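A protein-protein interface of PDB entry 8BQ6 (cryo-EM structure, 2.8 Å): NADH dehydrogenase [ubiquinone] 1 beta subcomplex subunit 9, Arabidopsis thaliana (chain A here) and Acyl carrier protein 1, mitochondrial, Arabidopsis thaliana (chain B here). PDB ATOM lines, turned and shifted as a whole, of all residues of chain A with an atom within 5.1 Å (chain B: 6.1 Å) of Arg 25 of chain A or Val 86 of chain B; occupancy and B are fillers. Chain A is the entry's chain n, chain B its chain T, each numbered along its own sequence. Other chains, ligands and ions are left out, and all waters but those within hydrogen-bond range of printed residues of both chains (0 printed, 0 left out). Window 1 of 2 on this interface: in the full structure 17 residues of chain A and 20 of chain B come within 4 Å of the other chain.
OE1 of Glu 84 of chain B is in hydrogen-bond range of OH of Tyr 24 of chain A (2.4 Å).
NH2 of Arg 25 of chain A is in salt-bridge range of OE1 of Glu 90 of chain B, 2.4 Å away.
The side-chain carboxylate of Glu 90 of chain B is in salt-bridge range of the side-chain amino group of Lys 29 of chain A, 3.1 Å away.
The backbone carbonyl oxygen (O) of Ile 97 of chain B sits at hydrogen-bond distance from the guanidinium group (NH2) of Arg 25 of chain A, 2.6 Å away.
The side-chain carboxylate (OD1) of Asp 99 of chain B lies within salt-bridge range of the guanidinium group (NE) of Arg 25 of chain A, at 3.0 Å.
The side-chain carboxylate (OD2) of Asp 99 of chain B is in salt-bridge range of the guanidinium group (NH1) of Arg 26 of chain A, at 3.1 Å.
The side-chain carboxylate (OD1) of Asp 103 of chain B lies within salt-bridge range of the guanidinium group (NH2) of Arg 21 of chain A.
N of Asp 81 of chain B sits close to OE2 of Glu 84 of chain B.
Ile 22 of chain A touches Asp 99 of chain B.
Asp 103 of chain B touches Ile 22 of chain A (OD2 to CG1, 3.3 Å).
CD1 of Tyr 24 of chain A touches CG2 of Val 83 of chain B, 3.5 Å away.
Arg 25 of chain A touches Val 86 of chain B (NH1 to CG1, 3.9 Å).
Arg 25 of chain A touches Ala 102 of chain B.
Leu 28 of chain A touches Glu 84 of chain B.
Met 87 of chain B touches Leu 28 of chain A (SD to CG, 3.9 Å).
Lys 29 of chain A touches Met 87 of chain B (CG to SD, 3.7 Å).
Of the printed residues of chain B, Tyr 24 of chain A touches Val 83 and Glu 84.
Arg 25 of chain A touches just these residues of chain B: Val 86 (3.9 Å), Glu 90 (2.4 Å), Ile 97 (2.6 Å), Asp 99 (3.0 Å) and Ala 102 (3.3 Å).
Printed residues of chain A within 4 Å of Glu 90 of chain B: Arg 25 (2.4 Å) and Lys 29 (3.1 Å).
Glu 91 of chain B touches none of the printed residues of chain A.
Asp 106 of chain B touches none of the printed residues of chain A.
The nearest printed residue of chain B that does not touch Ile 22 of chain A is Val 83 of chain B (5.6 Å).
Hydrophobic or aromatic side chains of chain B within 4 Å of the printed part of chain A: Val 83, Val 86, Met 87, Ile 97 and Ala 102.
Of the 10 printed residues of chain A, 7 touch a printed residue of chain B.
Hydrophobic or aromatic side chains of chain A within 4 Å of the printed part of chain B: Ile 22, Tyr 24 and Leu 28.
Among the printed residues, 15 pairs touch across the chains.
Among the printed residues, Asp or Glu carboxylates within 4 Å of a Lys or Arg side-chain nitrogen of the other chain: Arg 21 of chain A with Asp 103 of chain B (2.3 Å), Arg 25 of chain A with Glu 90 of chain B (2.4 Å), Arg 25 of chain A with Asp 99 of chain B (3.0 Å), Arg 26 of chain A with Asp 99 of chain B (3.1 Å) and Lys 29 of chain A with Glu 90 of chain B (3.1 Å).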
ATOM      1  N   VAL A  20     -34.049  19.314  20.636  1.00  0.00           N
ATOM      2  CA  VAL A  20     -32.733  19.929  20.487  1.00  0.00           C
ATOM      3  C   VAL A  20     -31.649  19.039  21.084  1.00  0.00           C
ATOM      4  O   VAL A  20     -30.590  18.832  20.480  1.00  0.00           O
ATOM      5  CB  VAL A  20     -32.720  21.329  21.127  1.00  0.00           C
ATOM      6  CG1 VAL A  20     -31.298  21.851  21.208  1.00  0.00           C
ATOM      7  CG2 VAL A  20     -33.591  22.284  20.334  1.00  0.00           C
ATOM      8  N   ARG A  21     -31.893  18.510  22.288  1.00  0.00           N
ATOM      9  CA  ARG A  21     -30.866  17.735  22.978  1.00  0.00           C
ATOM     10  C   ARG A  21     -30.518  16.471  22.207  1.00  0.00           C
ATOM     11  O   ARG A  21     -29.348  16.079  22.133  1.00  0.00           O
ATOM     12  CB  ARG A  21     -31.324  17.381  24.393  1.00  0.00           C
ATOM     13  CG  ARG A  21     -31.307  18.538  25.375  1.00  0.00           C
ATOM     14  CD  ARG A  21     -31.421  18.035  26.802  1.00  0.00           C
ATOM     15  NE  ARG A  21     -32.563  17.148  26.983  1.00  0.00           N
ATOM     16  CZ  ARG A  21     -33.760  17.549  27.384  1.00  0.00           C
ATOM     17  NH1 ARG A  21     -34.014  18.821  27.634  1.00  0.00           N
ATOM     18  NH2 ARG A  21     -34.729  16.650  27.535  1.00  0.00           N
ATOM     19  N   ILE A  22     -31.524  15.810  21.639  1.00  0.00           N
ATOM     20  CA  ILE A  22     -31.267  14.611  20.853  1.00  0.00           C
ATOM     21  C   ILE A  22     -30.544  14.955  19.558  1.00  0.00           C
ATOM     22  O   ILE A  22     -29.585  14.276  19.173  1.00  0.00           O
ATOM     23  CB  ILE A  22     -32.587  13.867  20.593  1.00  0.00           C
ATOM     24  CG1 ILE A  22     -33.025  13.135  21.862  1.00  0.00           C
ATOM     25  CG2 ILE A  22     -32.433  12.901  19.437  1.00  0.00           C
ATOM     26  CD1 ILE A  22     -34.509  12.899  21.948  1.00  0.00           C
ATOM     27  N   LEU A  23     -30.982  16.011  18.868  1.00  0.00           N
ATOM     28  CA  LEU A  23     -30.323  16.400  17.626  1.00  0.00           C
ATOM     29  C   LEU A  23     -28.861  16.750  17.872  1.00  0.00           C
ATOM     30  O   LEU A  23     -27.988  16.421  17.060  1.00  0.00           O
ATOM     31  CB  LEU A  23     -31.076  17.562  16.975  1.00  0.00           C
ATOM     32  CG  LEU A  23     -30.350  18.581  16.095  1.00  0.00           C
ATOM     33  CD1 LEU A  23     -29.785  17.943  14.838  1.00  0.00           C
ATOM     34  CD2 LEU A  23     -31.312  19.694  15.724  1.00  0.00           C
ATOM     35  N   TYR A  24     -28.567  17.403  19.001  1.00  0.00           N
ATOM     36  CA  TYR A  24     -27.172  17.627  19.366  1.00  0.00           C
ATOM     37  C   TYR A  24     -26.455  16.309  19.583  1.00  0.00           C
ATOM     38  O   TYR A  24     -25.323  16.123  19.124  1.00  0.00           O
ATOM     39  CB  TYR A  24     -27.074  18.500  20.620  1.00  0.00           C
ATOM     40  CG  TYR A  24     -25.647  18.876  20.995  1.00  0.00           C
ATOM     41  CD1 TYR A  24     -25.295  19.125  22.306  1.00  0.00           C
ATOM     42  CD2 TYR A  24     -24.643  18.940  20.030  1.00  0.00           C
ATOM     43  CE1 TYR A  24     -23.997  19.464  22.640  1.00  0.00           C
ATOM     44  CE2 TYR A  24     -23.361  19.280  20.350  1.00  0.00           C
ATOM     45  CZ  TYR A  24     -23.034  19.533  21.653  1.00  0.00           C
ATOM     46  OH  TYR A  24     -21.734  19.859  21.951  1.00  0.00           O
ATOM     47  N   ARG A  25     -27.110  15.376  20.265  1.00  0.00           N
ATOM     48  CA  ARG A  25     -26.502  14.077  20.502  1.00  0.00           C
ATOM     49  C   ARG A  25     -26.203  13.363  19.192  1.00  0.00           C
ATOM     50  O   ARG A  25     -25.126  12.783  19.025  1.00  0.00           O
ATOM     51  CB  ARG A  25     -27.423  13.235  21.374  1.00  0.00           C
ATOM     52  CG  ARG A  25     -27.036  11.801  21.410  1.00  0.00           C
ATOM     53  CD  ARG A  25     -27.678  11.105  22.566  1.00  0.00           C
ATOM     54  NE  ARG A  25     -27.557   9.666  22.403  1.00  0.00           N
ATOM     55  CZ  ARG A  25     -26.631   8.934  23.001  1.00  0.00           C
ATOM     56  NH1 ARG A  25     -25.729   9.479  23.800  1.00  0.00           N
ATOM     57  NH2 ARG A  25     -26.605   7.622  22.790  1.00  0.00           N
ATOM     58  N   ARG A  26     -27.138  13.405  18.245  1.00  0.00           N
ATOM     59  CA  ARG A  26     -26.925  12.704  16.986  1.00  0.00           C
ATOM     60  C   ARG A  26     -25.916  13.428  16.106  1.00  0.00           C
ATOM     61  O   ARG A  26     -25.051  12.791  15.492  1.00  0.00           O
ATOM     62  CB  ARG A  26     -28.250  12.527  16.257  1.00  0.00           C
ATOM     63  CG  ARG A  26     -28.774  11.121  16.361  1.00  0.00           C
ATOM     64  CD  ARG A  26     -29.758  10.831  15.265  1.00  0.00           C
ATOM     65  NE  ARG A  26     -30.922  11.701  15.323  1.00  0.00           N
ATOM     66  CZ  ARG A  26     -32.131  11.287  15.673  1.00  0.00           C
ATOM     67  NH1 ARG A  26     -32.357  10.029  16.013  1.00  0.00           N
ATOM     68  NH2 ARG A  26     -33.137  12.155  15.677  1.00  0.00           N
ATOM     69  N   ALA A  27     -26.008  14.755  16.028  1.00  0.00           N
ATOM     70  CA  ALA A  27     -25.060  15.511  15.217  1.00  0.00           C
ATOM     71  C   ALA A  27     -23.655  15.450  15.804  1.00  0.00           C
ATOM     72  O   ALA A  27     -22.666  15.566  15.072  1.00  0.00           O
ATOM     73  CB  ALA A  27     -25.526  16.959  15.078  1.00  0.00           C
ATOM     74  N   LEU A  28     -23.544  15.274  17.122  1.00  0.00           N
ATOM     75  CA  LEU A  28     -22.221  15.185  17.733  1.00  0.00           C
ATOM     76  C   LEU A  28     -21.567  13.843  17.443  1.00  0.00           C
ATOM     77  O   LEU A  28     -20.350  13.771  17.240  1.00  0.00           O
ATOM     78  CB  LEU A  28     -22.312  15.423  19.238  1.00  0.00           C
ATOM     79  CG  LEU A  28     -21.027  15.882  19.925  1.00  0.00           C
ATOM     80  CD1 LEU A  28     -20.350  16.973  19.123  1.00  0.00           C
ATOM     81  CD2 LEU A  28     -21.347  16.373  21.317  1.00  0.00           C
ATOM     82  N   LYS A  29     -22.353  12.763  17.430  1.00  0.00           N
ATOM     83  CA  LYS A  29     -21.782  11.462  17.102  1.00  0.00           C
ATOM     84  C   LYS A  29     -21.452  11.359  15.620  1.00  0.00           C
ATOM     85  O   LYS A  29     -20.413  10.796  15.257  1.00  0.00           O
ATOM     86  CB  LYS A  29     -22.728  10.341  17.530  1.00  0.00           C
ATOM     87  CG  LYS A  29     -22.980  10.308  19.029  1.00  0.00           C
ATOM     88  CD  LYS A  29     -23.860   9.146  19.438  1.00  0.00           C
ATOM     89  CE  LYS A  29     -23.112   7.839  19.306  1.00  0.00           C
ATOM     90  NZ  LYS A  29     -22.011   7.716  20.289  1.00  0.00           N
ATOM     91  N   PHE B  71     -26.438  17.202  37.176  1.00  0.00           N
ATOM     92  CA  PHE B  71     -25.536  18.022  36.327  1.00  0.00           C
ATOM     93  C   PHE B  71     -26.040  19.462  36.190  1.00  0.00           C
ATOM     94  O   PHE B  71     -25.217  20.383  36.315  1.00  0.00           O
ATOM     95  CB  PHE B  71     -25.394  17.371  34.952  1.00  0.00           C
ATOM     96  CG  PHE B  71     -24.886  15.950  34.964  1.00  0.00           C
ATOM     97  CD1 PHE B  71     -23.839  15.575  35.789  1.00  0.00           C
ATOM     98  CD2 PHE B  71     -25.453  14.989  34.143  1.00  0.00           C
ATOM     99  CE1 PHE B  71     -23.375  14.269  35.796  1.00  0.00           C
ATOM    100  CE2 PHE B  71     -24.992  13.683  34.153  1.00  0.00           C
ATOM    101  CZ  PHE B  71     -23.953  13.327  34.978  1.00  0.00           C
ATOM    102  N   ASP B  81     -24.405  20.597  27.857  1.00  0.00           N
ATOM    103  CA  ASP B  81     -23.256  20.076  28.592  1.00  0.00           C
ATOM    104  C   ASP B  81     -23.514  18.661  29.089  1.00  0.00           C
ATOM    105  O   ASP B  81     -22.589  17.844  29.162  1.00  0.00           O
ATOM    106  CB  ASP B  81     -22.904  21.010  29.743  1.00  0.00           C
ATOM    107  CG  ASP B  81     -22.436  22.358  29.258  1.00  0.00           C
ATOM    108  OD1 ASP B  81     -21.229  22.654  29.367  1.00  0.00           O
ATOM    109  OD2 ASP B  81     -23.280  23.114  28.734  1.00  0.00           O
ATOM    110  N   THR B  82     -24.772  18.342  29.409  1.00  0.00           N
ATOM    111  CA  THR B  82     -25.077  16.992  29.962  1.00  0.00           C
ATOM    112  C   THR B  82     -24.936  15.926  28.866  1.00  0.00           C
ATOM    113  O   THR B  82     -24.410  14.858  29.192  1.00  0.00           O
ATOM    114  CB  THR B  82     -26.445  16.913  30.660  1.00  0.00           C
ATOM    115  OG1 THR B  82     -27.491  16.807  29.692  1.00  0.00           O
ATOM    116  CG2 THR B  82     -26.710  18.089  31.574  1.00  0.00           C
ATOM    117  N   VAL B  83     -25.376  16.193  27.629  1.00  0.00           N
ATOM    118  CA  VAL B  83     -25.324  15.147  26.612  1.00  0.00           C
ATOM    119  C   VAL B  83     -23.882  14.839  26.224  1.00  0.00           C
ATOM    120  O   VAL B  83     -23.565  13.708  25.839  1.00  0.00           O
ATOM    121  CB  VAL B  83     -26.184  15.509  25.385  1.00  0.00           C
ATOM    122  CG1 VAL B  83     -27.652  15.240  25.675  1.00  0.00           C
ATOM    123  CG2 VAL B  83     -25.979  16.936  24.964  1.00  0.00           C
ATOM    124  N   GLU B  84     -22.980  15.823  26.320  1.00  0.00           N
ATOM    125  CA  GLU B  84     -21.571  15.502  26.103  1.00  0.00           C
ATOM    126  C   GLU B  84     -21.039  14.598  27.201  1.00  0.00           C
ATOM    127  O   GLU B  84     -20.209  13.719  26.943  1.00  0.00           O
ATOM    128  CB  GLU B  84     -20.702  16.755  26.013  1.00  0.00           C
ATOM    129  CG  GLU B  84     -20.923  17.626  24.801  1.00  0.00           C
ATOM    130  CD  GLU B  84     -21.507  18.966  25.151  1.00  0.00           C
ATOM    131  OE1 GLU B  84     -21.364  19.920  24.368  1.00  0.00           O
ATOM    132  OE2 GLU B  84     -22.070  19.076  26.227  1.00  0.00           O
ATOM    133  N   ILE B  85     -21.484  14.839  28.438  1.00  0.00           N
ATOM    134  CA  ILE B  85     -21.080  13.951  29.567  1.00  0.00           C
ATOM    135  C   ILE B  85     -21.637  12.553  29.275  1.00  0.00           C
ATOM    136  O   ILE B  85     -20.879  11.587  29.430  1.00  0.00           O
ATOM    137  CB  ILE B  85     -21.566  14.525  30.915  1.00  0.00           C
ATOM    138  CG1 ILE B  85     -20.863  15.841  31.254  1.00  0.00           C
ATOM    139  CG2 ILE B  85     -21.413  13.517  32.041  1.00  0.00           C
ATOM    140  CD1 ILE B  85     -21.464  16.570  32.432  1.00  0.00           C
ATOM    141  N   VAL B  86     -22.891  12.461  28.817  1.00  0.00           N
ATOM    142  CA  VAL B  86     -23.497  11.177  28.492  1.00  0.00           C
ATOM    143  C   VAL B  86     -22.730  10.495  27.362  1.00  0.00           C
ATOM    144  O   VAL B  86     -22.621   9.264  27.323  1.00  0.00           O
ATOM    145  CB  VAL B  86     -24.985  11.388  28.155  1.00  0.00           C
ATOM    146  CG1 VAL B  86     -25.625  10.115  27.628  1.00  0.00           C
ATOM    147  CG2 VAL B  86     -25.728  11.896  29.386  1.00  0.00           C
ATOM    148  N   MET B  87     -22.166  11.286  26.442  1.00  0.00           N
ATOM    149  CA  MET B  87     -21.388  10.723  25.340  1.00  0.00           C
ATOM    150  C   MET B  87     -20.003  10.284  25.800  1.00  0.00           C
ATOM    151  O   MET B  87     -19.439   9.322  25.263  1.00  0.00           O
ATOM    152  CB  MET B  87     -21.273  11.743  24.209  1.00  0.00           C
ATOM    153  CG  MET B  87     -21.578  11.183  22.832  1.00  0.00           C
ATOM    154  SD  MET B  87     -21.094  12.292  21.495  1.00  0.00           S
ATOM    155  CE  MET B  87     -19.317  12.076  21.515  1.00  0.00           C
ATOM    156  N   ALA B  88     -19.421  10.996  26.766  1.00  0.00           N
ATOM    157  CA  ALA B  88     -18.161  10.547  27.346  1.00  0.00           C
ATOM    158  C   ALA B  88     -18.368   9.314  28.214  1.00  0.00           C
ATOM    159  O   ALA B  88     -17.509   8.427  28.260  1.00  0.00           O
ATOM    160  CB  ALA B  88     -17.521  11.673  28.156  1.00  0.00           C
ATOM    161  N   ILE B  89     -19.497   9.248  28.920  1.00  0.00           N
ATOM    162  CA  ILE B  89     -19.833   8.033  29.656  1.00  0.00           C
ATOM    163  C   ILE B  89     -20.067   6.886  28.684  1.00  0.00           C
ATOM    164  O   ILE B  89     -19.763   5.724  28.982  1.00  0.00           O
ATOM    165  CB  ILE B  89     -21.046   8.284  30.571  1.00  0.00           C
ATOM    166  CG1 ILE B  89     -20.623   9.123  31.774  1.00  0.00           C
ATOM    167  CG2 ILE B  89     -21.666   6.978  31.048  1.00  0.00           C
ATOM    168  CD1 ILE B  89     -21.764   9.830  32.446  1.00  0.00           C
ATOM    169  N   GLU B  90     -20.590   7.196  27.497  1.00  0.00           N
ATOM    170  CA  GLU B  90     -20.755   6.175  26.470  1.00  0.00           C
ATOM    171  C   GLU B  90     -19.422   5.589  26.039  1.00  0.00           C
ATOM    172  O   GLU B  90     -19.252   4.365  26.007  1.00  0.00           O
ATOM    173  CB  GLU B  90     -21.483   6.763  25.268  1.00  0.00           C
ATOM    174  CG  GLU B  90     -22.836   6.173  25.086  1.00  0.00           C
ATOM    175  CD  GLU B  90     -23.715   6.986  24.186  1.00  0.00           C
ATOM    176  OE1 GLU B  90     -24.923   7.070  24.481  1.00  0.00           O
ATOM    177  OE2 GLU B  90     -23.210   7.534  23.186  1.00  0.00           O
ATOM    178  N   GLU B  91     -18.464   6.448  25.700  1.00  0.00           N
ATOM    179  CA  GLU B  91     -17.157   5.977  25.265  1.00  0.00           C
ATOM    180  C   GLU B  91     -16.376   5.323  26.394  1.00  0.00           C
ATOM    181  O   GLU B  91     -15.493   4.499  26.133  1.00  0.00           O
ATOM    182  CB  GLU B  91     -16.354   7.138  24.690  1.00  0.00           C
ATOM    183  CG  GLU B  91     -15.239   6.711  23.776  1.00  0.00           C
ATOM    184  CD  GLU B  91     -15.018   7.691  22.650  1.00  0.00           C
ATOM    185  OE1 GLU B  91     -14.177   7.410  21.772  1.00  0.00           O
ATOM    186  OE2 GLU B  91     -15.689   8.745  22.643  1.00  0.00           O
ATOM    187  N   GLU B  96     -23.791   1.778  23.589  1.00  0.00           N
ATOM    188  CA  GLU B  96     -24.605   2.511  22.625  1.00  0.00           C
ATOM    189  C   GLU B  96     -25.984   2.689  23.250  1.00  0.00           C
ATOM    190  O   GLU B  96     -26.870   1.848  23.082  1.00  0.00           O
ATOM    191  CB  GLU B  96     -24.686   1.797  21.274  1.00  0.00           C
ATOM    192  CG  GLU B  96     -25.310   2.662  20.188  1.00  0.00           C
ATOM    193  CD  GLU B  96     -24.719   2.436  18.804  1.00  0.00           C
ATOM    194  OE1 GLU B  96     -23.483   2.312  18.679  1.00  0.00           O
ATOM    195  OE2 GLU B  96     -25.499   2.405  17.831  1.00  0.00           O
ATOM    196  N   ILE B  97     -26.156   3.781  23.980  1.00  0.00           N
ATOM    197  CA  ILE B  97     -27.439   4.076  24.619  1.00  0.00           C
ATOM    198  C   ILE B  97     -28.407   4.600  23.563  1.00  0.00           C
ATOM    199  O   ILE B  97     -28.038   5.497  22.789  1.00  0.00           O
ATOM    200  CB  ILE B  97     -27.256   5.084  25.749  1.00  0.00           C
ATOM    201  CG1 ILE B  97     -26.582   4.418  26.948  1.00  0.00           C
ATOM    202  CG2 ILE B  97     -28.588   5.655  26.178  1.00  0.00           C
ATOM    203  CD1 ILE B  97     -25.119   4.721  27.108  1.00  0.00           C
ATOM    204  N   PRO B  98     -29.623   4.066  23.487  1.00  0.00           N
ATOM    205  CA  PRO B  98     -30.619   4.631  22.573  1.00  0.00           C
ATOM    206  C   PRO B  98     -30.894   6.093  22.889  1.00  0.00           C
ATOM    207  O   PRO B  98     -30.885   6.513  24.049  1.00  0.00           O
ATOM    208  CB  PRO B  98     -31.856   3.765  22.821  1.00  0.00           C
ATOM    209  CG  PRO B  98     -31.311   2.487  23.320  1.00  0.00           C
ATOM    210  CD  PRO B  98     -30.107   2.835  24.133  1.00  0.00           C
ATOM    211  N   ASP B  99     -31.147   6.867  21.829  1.00  0.00           N
ATOM    212  CA  ASP B  99     -31.298   8.313  21.967  1.00  0.00           C
ATOM    213  C   ASP B  99     -32.389   8.682  22.965  1.00  0.00           C
ATOM    214  O   ASP B  99     -32.290   9.717  23.634  1.00  0.00           O
ATOM    215  CB  ASP B  99     -31.608   8.940  20.608  1.00  0.00           C
ATOM    216  CG  ASP B  99     -30.434   8.876  19.641  1.00  0.00           C
ATOM    217  OD1 ASP B  99     -29.269   8.807  20.087  1.00  0.00           O
ATOM    218  OD2 ASP B  99     -30.688   8.889  18.419  1.00  0.00           O
ATOM    219  N   ALA B 102     -30.931   8.140  26.438  1.00  0.00           N
ATOM    220  CA  ALA B 102     -29.813   9.047  26.668  1.00  0.00           C
ATOM    221  C   ALA B 102     -30.294  10.409  27.148  1.00  0.00           C
ATOM    222  O   ALA B 102     -29.631  11.059  27.964  1.00  0.00           O
ATOM    223  CB  ALA B 102     -28.989   9.193  25.392  1.00  0.00           C
ATOM    224  N   ASP B 103     -31.442  10.864  26.645  1.00  0.00           N
ATOM    225  CA  ASP B 103     -31.938  12.180  27.024  1.00  0.00           C
ATOM    226  C   ASP B 103     -32.564  12.187  28.408  1.00  0.00           C
ATOM    227  O   ASP B 103     -32.793  13.265  28.965  1.00  0.00           O
ATOM    228  CB  ASP B 103     -32.954  12.681  26.002  1.00  0.00           C
ATOM    229  CG  ASP B 103     -32.878  14.179  25.805  1.00  0.00           C
ATOM    230  OD1 ASP B 103     -32.312  14.861  26.684  1.00  0.00           O
ATOM    231  OD2 ASP B 103     -33.397  14.675  24.787  1.00  0.00           O
ATOM    232  N   ILE B 105     -31.120  10.705  31.062  1.00  0.00           N
ATOM    233  CA  ILE B 105     -30.043  10.713  32.047  1.00  0.00           C
ATOM    234  C   ILE B 105     -29.593  12.142  32.320  1.00  0.00           C
ATOM    235  O   ILE B 105     -28.965  12.785  31.470  1.00  0.00           O
ATOM    236  CB  ILE B 105     -28.866   9.829  31.595  1.00  0.00           C
ATOM    237  CG1 ILE B 105     -29.339   8.382  31.440  1.00  0.00           C
ATOM    238  CG2 ILE B 105     -27.727   9.911  32.592  1.00  0.00           C
ATOM    239  CD1 ILE B 105     -28.491   7.534  30.531  1.00  0.00           C
ATOM    240  N   ASP B 106     -29.906  12.657  33.513  1.00  0.00           N
ATOM    241  CA  ASP B 106     -29.562  14.074  33.819  1.00  0.00           C
ATOM    242  C   ASP B 106     -28.851  14.180  35.175  1.00  0.00           C
ATOM    243  O   ASP B 106     -28.463  15.308  35.541  1.00  0.00           O
ATOM    244  CB  ASP B 106     -30.801  14.971  33.723  1.00  0.00           C
ATOM    245  CG  ASP B 106     -31.166  15.321  32.291  1.00  0.00           C
ATOM    246  OD1 ASP B 106     -30.364  16.016  31.636  1.00  0.00           O
ATOM    247  OD2 ASP B 106     -32.241  14.882  31.838  1.00  0.00           O
